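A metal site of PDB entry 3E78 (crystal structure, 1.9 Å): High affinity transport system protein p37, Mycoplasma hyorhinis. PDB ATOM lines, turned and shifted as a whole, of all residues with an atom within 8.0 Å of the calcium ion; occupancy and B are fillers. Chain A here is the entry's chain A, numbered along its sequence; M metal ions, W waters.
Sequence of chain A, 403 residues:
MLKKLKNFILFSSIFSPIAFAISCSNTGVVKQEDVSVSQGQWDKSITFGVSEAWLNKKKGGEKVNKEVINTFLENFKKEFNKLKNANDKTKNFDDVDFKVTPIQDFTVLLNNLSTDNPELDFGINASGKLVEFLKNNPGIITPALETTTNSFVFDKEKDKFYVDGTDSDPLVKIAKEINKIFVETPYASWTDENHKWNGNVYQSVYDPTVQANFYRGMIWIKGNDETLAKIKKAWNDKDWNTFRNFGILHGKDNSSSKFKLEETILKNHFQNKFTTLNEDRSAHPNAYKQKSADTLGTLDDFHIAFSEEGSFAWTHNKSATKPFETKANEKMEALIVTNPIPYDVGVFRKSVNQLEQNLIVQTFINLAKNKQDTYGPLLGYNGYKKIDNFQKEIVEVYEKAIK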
ATOM      1  N   TRP A  42     -21.279 -23.994  15.944  1.00  0.00           N
ATOM      2  CA  TRP A  42     -20.579 -23.577  14.739  1.00  0.00           C
ATOM      3  C   TRP A  42     -21.479 -23.699  13.513  1.00  0.00           C
ATOM      4  O   TRP A  42     -21.980 -24.785  13.219  1.00  0.00           O
ATOM      5  CB  TRP A  42     -19.317 -24.411  14.513  1.00  0.00           C
ATOM      6  CG  TRP A  42     -18.403 -23.826  13.474  1.00  0.00           C
ATOM      7  CD1 TRP A  42     -18.374 -24.125  12.146  1.00  0.00           C
ATOM      8  CD2 TRP A  42     -17.406 -22.827  13.689  1.00  0.00           C
ATOM      9  NE1 TRP A  42     -17.408 -23.376  11.507  1.00  0.00           N
ATOM     10  CE2 TRP A  42     -16.791 -22.579  12.441  1.00  0.00           C
ATOM     11  CE3 TRP A  42     -16.956 -22.137  14.817  1.00  0.00           C
ATOM     12  CZ2 TRP A  42     -15.761 -21.647  12.301  1.00  0.00           C
ATOM     13  CZ3 TRP A  42     -15.933 -21.217  14.672  1.00  0.00           C
ATOM     14  CH2 TRP A  42     -15.351 -20.985  13.426  1.00  0.00           C
ATOM     15  N   ASP A  43     -21.692 -22.582  12.824  1.00  0.00           N
ATOM     16  CA  ASP A  43     -22.570 -22.568  11.639  1.00  0.00           C
ATOM     17  C   ASP A  43     -21.743 -22.381  10.380  1.00  0.00           C
ATOM     18  O   ASP A  43     -21.097 -21.337  10.189  1.00  0.00           O
ATOM     19  CB  ASP A  43     -23.615 -21.478  11.827  1.00  0.00           C
ATOM     20  CG  ASP A  43     -24.701 -21.466  10.771  1.00  0.00           C
ATOM     21  OD1 ASP A  43     -24.640 -22.287   9.827  1.00  0.00           O
ATOM     22  OD2 ASP A  43     -25.756 -20.837  11.022  1.00  0.00           O
ATOM     23  N   LYS A  44     -21.709 -23.382   9.502  1.00  0.00           N
ATOM     24  CA  LYS A  44     -20.820 -23.318   8.340  1.00  0.00           C
ATOM     25  C   LYS A  44     -21.400 -22.394   7.265  1.00  0.00           C
ATOM     26  O   LYS A  44     -20.778 -22.099   6.241  1.00  0.00           O
ATOM     27  CB  LYS A  44     -20.566 -24.711   7.756  1.00  0.00           C
ATOM     28  CG  LYS A  44     -21.704 -25.254   6.911  1.00  0.00           C
ATOM     29  CD  LYS A  44     -21.436 -26.700   6.509  1.00  0.00           C
ATOM     30  CE  LYS A  44     -21.347 -26.882   5.012  1.00  0.00           C
ATOM     31  NZ  LYS A  44     -20.219 -27.767   4.585  1.00  0.00           N
ATOM     32  N   SER A  45     -22.606 -21.906   7.499  1.00  0.00           N
ATOM     33  CA  SER A  45     -23.181 -20.954   6.554  1.00  0.00           C
ATOM     34  C   SER A  45     -23.702 -19.748   7.350  1.00  0.00           C
ATOM     35  O   SER A  45     -24.576 -19.884   8.192  1.00  0.00           O
ATOM     36  CB  SER A  45     -24.293 -21.584   5.734  1.00  0.00           C
ATOM     37  OG  SER A  45     -25.335 -20.655   5.462  1.00  0.00           O
ATOM     38  N   ILE A  46     -23.136 -18.575   7.053  1.00  0.00           N
ATOM     39  CA  ILE A  46     -23.551 -17.400   7.833  1.00  0.00           C
ATOM     40  C   ILE A  46     -24.270 -16.435   6.916  1.00  0.00           C
ATOM     41  O   ILE A  46     -23.746 -16.076   5.861  1.00  0.00           O
ATOM     42  CB  ILE A  46     -22.320 -16.764   8.499  1.00  0.00           C
ATOM     43  CG1 ILE A  46     -21.851 -17.540   9.728  1.00  0.00           C
ATOM     44  CG2 ILE A  46     -22.559 -15.290   8.817  1.00  0.00           C
ATOM     45  CD1 ILE A  46     -22.822 -17.578  10.885  1.00  0.00           C
ATOM     46  N   THR A  47     -25.482 -16.033   7.273  1.00  0.00           N
ATOM     47  CA  THR A  47     -26.222 -15.134   6.394  1.00  0.00           C
ATOM     48  C   THR A  47     -26.401 -13.758   7.038  1.00  0.00           C
ATOM     49  O   THR A  47     -26.927 -13.660   8.137  1.00  0.00           O
ATOM     50  CB  THR A  47     -27.603 -15.725   6.097  1.00  0.00           C
ATOM     51  OG1 THR A  47     -27.445 -16.982   5.411  1.00  0.00           O
ATOM     52  CG2 THR A  47     -28.393 -14.795   5.173  1.00  0.00           C
ATOM     53  N   PHE A  48     -26.000 -12.688   6.358  1.00  0.00           N
ATOM     54  CA  PHE A  48     -26.258 -11.333   6.833  1.00  0.00           C
ATOM     55  C   PHE A  48     -27.581 -10.778   6.310  1.00  0.00           C
ATOM     56  O   PHE A  48     -27.887 -10.920   5.122  1.00  0.00           O
ATOM     57  CB  PHE A  48     -25.164 -10.371   6.378  1.00  0.00           C
ATOM     58  CG  PHE A  48     -23.749 -10.783   6.728  1.00  0.00           C
ATOM     59  CD1 PHE A  48     -23.466 -11.279   7.997  1.00  0.00           C
ATOM     60  CD2 PHE A  48     -22.721 -10.657   5.818  1.00  0.00           C
ATOM     61  CE1 PHE A  48     -22.178 -11.643   8.332  1.00  0.00           C
ATOM     62  CE2 PHE A  48     -21.424 -11.019   6.135  1.00  0.00           C
ATOM     63  CZ  PHE A  48     -21.158 -11.498   7.408  1.00  0.00           C
ATOM     64  N   VAL A  96     -16.353 -21.568   6.434  1.00  0.00           N
ATOM     65  CA  VAL A  96     -17.664 -20.952   6.459  1.00  0.00           C
ATOM     66  C   VAL A  96     -17.966 -20.185   5.180  1.00  0.00           C
ATOM     67  O   VAL A  96     -17.115 -19.491   4.622  1.00  0.00           O
ATOM     68  CB  VAL A  96     -17.771 -20.004   7.679  1.00  0.00           C
ATOM     69  CG1 VAL A  96     -19.137 -19.338   7.726  1.00  0.00           C
ATOM     70  CG2 VAL A  96     -17.534 -20.744   8.984  1.00  0.00           C
ATOM     71  N   ASP A  97     -19.200 -20.296   4.690  1.00  0.00           N
ATOM     72  CA  ASP A  97     -19.610 -19.511   3.539  1.00  0.00           C
ATOM     73  C   ASP A  97     -20.456 -18.339   4.012  1.00  0.00           C
ATOM     74  O   ASP A  97     -21.147 -18.485   5.029  1.00  0.00           O
ATOM     75  CB  ASP A  97     -20.440 -20.359   2.567  1.00  0.00           C
ATOM     76  CG  ASP A  97     -19.496 -21.104   1.630  1.00  0.00           C
ATOM     77  OD1 ASP A  97     -18.725 -20.421   0.925  1.00  0.00           O
ATOM     78  OD2 ASP A  97     -19.524 -22.351   1.620  1.00  0.00           O
ATOM     79  N   LYS A  99     -23.421 -15.355   2.963  1.00  0.00           N
ATOM     80  CA  LYS A  99     -24.475 -14.913   2.090  1.00  0.00           C
ATOM     81  C   LYS A  99     -25.190 -13.709   2.692  1.00  0.00           C
ATOM     82  O   LYS A  99     -25.049 -13.395   3.873  1.00  0.00           O
ATOM     83  CB  LYS A  99     -25.516 -16.022   1.884  1.00  0.00           C
ATOM     84  CG  LYS A  99     -24.936 -17.430   1.912  1.00  0.00           C
ATOM     85  CD  LYS A  99     -25.996 -18.481   1.681  1.00  0.00           C
ATOM     86  CE  LYS A  99     -27.004 -18.557   2.813  1.00  0.00           C
ATOM     87  NZ  LYS A  99     -28.316 -17.923   2.476  1.00  0.00           N
ATOM     88  N   ASN A 117     -32.847 -18.495  14.273  1.00  0.00           N
ATOM     89  CA  ASN A 117     -32.908 -19.354  13.101  1.00  0.00           C
ATOM     90  C   ASN A 117     -31.663 -19.199  12.228  1.00  0.00           C
ATOM     91  O   ASN A 117     -31.251 -18.093  11.854  1.00  0.00           O
ATOM     92  CB  ASN A 117     -34.165 -19.004  12.292  1.00  0.00           C
ATOM     93  CG  ASN A 117     -34.571 -20.128  11.373  1.00  0.00           C
ATOM     94  OD1 ASN A 117     -33.781 -20.558  10.530  1.00  0.00           O
ATOM     95  ND2 ASN A 117     -35.792 -20.608  11.525  1.00  0.00           N
ATOM     96  N   PRO A 118     -31.020 -20.300  11.873  1.00  0.00           N
ATOM     97  CA  PRO A 118     -29.794 -20.252  11.090  1.00  0.00           C
ATOM     98  C   PRO A 118     -29.953 -19.669   9.693  1.00  0.00           C
ATOM     99  O   PRO A 118     -28.941 -19.450   9.013  1.00  0.00           O
ATOM    100  CB  PRO A 118     -29.384 -21.729  10.964  1.00  0.00           C
ATOM    101  CG  PRO A 118     -30.082 -22.388  12.118  1.00  0.00           C
ATOM    102  CD  PRO A 118     -31.402 -21.684  12.217  1.00  0.00           C
ATOM    103  N   GLU A 119     -31.189 -19.425   9.258  1.00  0.00           N
ATOM    104  CA  GLU A 119     -31.397 -18.741   7.983  1.00  0.00           C
ATOM    105  C   GLU A 119     -30.980 -17.260   8.112  1.00  0.00           C
ATOM    106  O   GLU A 119     -30.768 -16.585   7.103  1.00  0.00           O
ATOM    107  CB  GLU A 119     -32.838 -18.800   7.493  1.00  0.00           C
ATOM    108  CG  GLU A 119     -33.938 -18.656   8.490  1.00  0.00           C
ATOM    109  CD  GLU A 119     -34.736 -17.383   8.547  1.00  0.00           C
ATOM    110  OE1 GLU A 119     -34.978 -16.753   7.498  1.00  0.00           O
ATOM    111  OE2 GLU A 119     -35.160 -16.981   9.658  1.00  0.00           O
ATOM    112  N   LEU A 120     -30.861 -16.768   9.337  1.00  0.00           N
ATOM    113  CA  LEU A 120     -30.498 -15.370   9.530  1.00  0.00           C
ATOM    114  C   LEU A 120     -29.699 -15.249  10.815  1.00  0.00           C
ATOM    115  O   LEU A 120     -30.218 -15.424  11.907  1.00  0.00           O
ATOM    116  CB  LEU A 120     -31.738 -14.476   9.569  1.00  0.00           C
ATOM    117  CG  LEU A 120     -31.440 -12.978   9.763  1.00  0.00           C
ATOM    118  CD1 LEU A 120     -30.754 -12.411   8.534  1.00  0.00           C
ATOM    119  CD2 LEU A 120     -32.729 -12.233  10.065  1.00  0.00           C
ATOM    120  N   ASP A 121     -28.402 -14.997  10.618  1.00  0.00           N
ATOM    121  CA  ASP A 121     -27.460 -15.028  11.710  1.00  0.00           C
ATOM    122  C   ASP A 121     -27.086 -13.645  12.224  1.00  0.00           C
ATOM    123  O   ASP A 121     -26.706 -13.530  13.392  1.00  0.00           O
ATOM    124  CB  ASP A 121     -26.163 -15.717  11.248  1.00  0.00           C
ATOM    125  CG  ASP A 121     -26.449 -17.091  10.633  1.00  0.00           C
ATOM    126  OD1 ASP A 121     -26.341 -17.224   9.401  1.00  0.00           O
ATOM    127  OD2 ASP A 121     -27.046 -17.864  11.406  1.00  0.00           O
ATOM    128  N   PHE A 122     -27.152 -12.610  11.397  1.00  0.00           N
ATOM    129  CA  PHE A 122     -26.508 -11.356  11.776  1.00  0.00           C
ATOM    130  C   PHE A 122     -27.111 -10.190  11.002  1.00  0.00           C
ATOM    131  O   PHE A 122     -27.515 -10.372   9.859  1.00  0.00           O
ATOM    132  CB  PHE A 122     -25.008 -11.441  11.484  1.00  0.00           C
ATOM    133  CG  PHE A 122     -24.202 -10.185  11.755  1.00  0.00           C
ATOM    134  CD1 PHE A 122     -23.647  -9.977  13.015  1.00  0.00           C
ATOM    135  CD2 PHE A 122     -23.983  -9.214  10.786  1.00  0.00           C
ATOM    136  CE1 PHE A 122     -22.909  -8.846  13.303  1.00  0.00           C
ATOM    137  CE2 PHE A 122     -23.249  -8.083  11.061  1.00  0.00           C
ATOM    138  CZ  PHE A 122     -22.706  -7.908  12.310  1.00  0.00           C
ATOM    139  N   ARG A 349     -27.857 -13.621  16.162  1.00  0.00           N
ATOM    140  CA  ARG A 349     -28.789 -14.488  16.884  1.00  0.00           C
ATOM    141  C   ARG A 349     -27.973 -15.173  17.976  1.00  0.00           C
ATOM    142  O   ARG A 349     -26.739 -15.263  17.920  1.00  0.00           O
ATOM    143  CB  ARG A 349     -29.461 -15.479  15.943  1.00  0.00           C
ATOM    144  CG  ARG A 349     -28.465 -16.456  15.323  1.00  0.00           C
ATOM    145  CD  ARG A 349     -29.125 -17.413  14.370  1.00  0.00           C
ATOM    146  NE  ARG A 349     -28.157 -18.220  13.619  1.00  0.00           N
ATOM    147  CZ  ARG A 349     -27.804 -19.416  14.100  1.00  0.00           C
ATOM    148  NH1 ARG A 349     -28.358 -19.824  15.247  1.00  0.00           N
ATOM    149  NH2 ARG A 349     -26.944 -20.174  13.446  1.00  0.00           N
ATOM    150  N   VAL A 352     -25.205 -18.560  17.658  1.00  0.00           N
ATOM    151  CA  VAL A 352     -23.995 -18.616  16.854  1.00  0.00           C
ATOM    152  C   VAL A 352     -22.794 -18.807  17.778  1.00  0.00           C
ATOM    153  O   VAL A 352     -22.681 -18.097  18.777  1.00  0.00           O
ATOM    154  CB  VAL A 352     -23.766 -17.341  16.041  1.00  0.00           C
ATOM    155  CG1 VAL A 352     -22.381 -17.338  15.405  1.00  0.00           C
ATOM    156  CG2 VAL A 352     -24.850 -17.217  14.988  1.00  0.00           C
ATOM    157  N   GLU A 356     -16.913 -18.162  16.681  1.00  0.00           N
ATOM    158  CA  GLU A 356     -17.272 -17.760  15.328  1.00  0.00           C
ATOM    159  C   GLU A 356     -17.661 -16.276  15.307  1.00  0.00           C
ATOM    160  O   GLU A 356     -17.281 -15.581  14.365  1.00  0.00           O
ATOM    161  CB  GLU A 356     -18.414 -18.616  14.782  1.00  0.00           C
ATOM    162  CG  GLU A 356     -18.653 -18.432  13.283  1.00  0.00           C
ATOM    163  CD  GLU A 356     -19.624 -19.437  12.683  1.00  0.00           C
ATOM    164  OE1 GLU A 356     -20.352 -20.113  13.434  1.00  0.00           O
ATOM    165  OE2 GLU A 356     -19.689 -19.542  11.444  1.00  0.00           O
HETATM  166 CA    CA M   1     -26.677 -19.546   9.291  1.00  0.00          CA
HETATM  167  O   HOH W   1     -27.150 -19.247   6.683  1.00  0.00           O
HETATM  168  O   HOH W   2     -26.914 -22.398   8.326  1.00  0.00           O
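The calcium ion is bound by the backbone carbonyl oxygen (O) of Pro 118, the side-chain carboxylate (OD2) of Asp 43, the side-chain carboxylate (OD1) of Asp 121, the backbone carbonyl oxygen (O) of Ser 45, water W1 and the side-chain carboxylate (OD2) of Asp 121.
The calcium ion has six donor atoms within binding distance.
Slightly farther from the calcium ion lies water W2 (3.0 Å).
Water W1 bridges OG of Ser 45 (2.6 Å) and OG1 of Thr 47 (2.6 Å).
Of the 19 residues printed, 4 come within 4 Å of the calcium ion.
The side-chain carboxylate (OD2) of Asp 43 lies close to the guanidinium group (NH2) of Arg 349.
N of Asp 43 is in hydrogen-bond range of OE1 of Glu 356.
The backbone carbonyl oxygen (O) of Asp 121 sits at hydrogen-bond distance from the backbone NH (N) of Arg 349, at 3.0 Å.
N of Asp 121 sits at hydrogen-bond distance from O of Thr 47 (3.2 Å).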
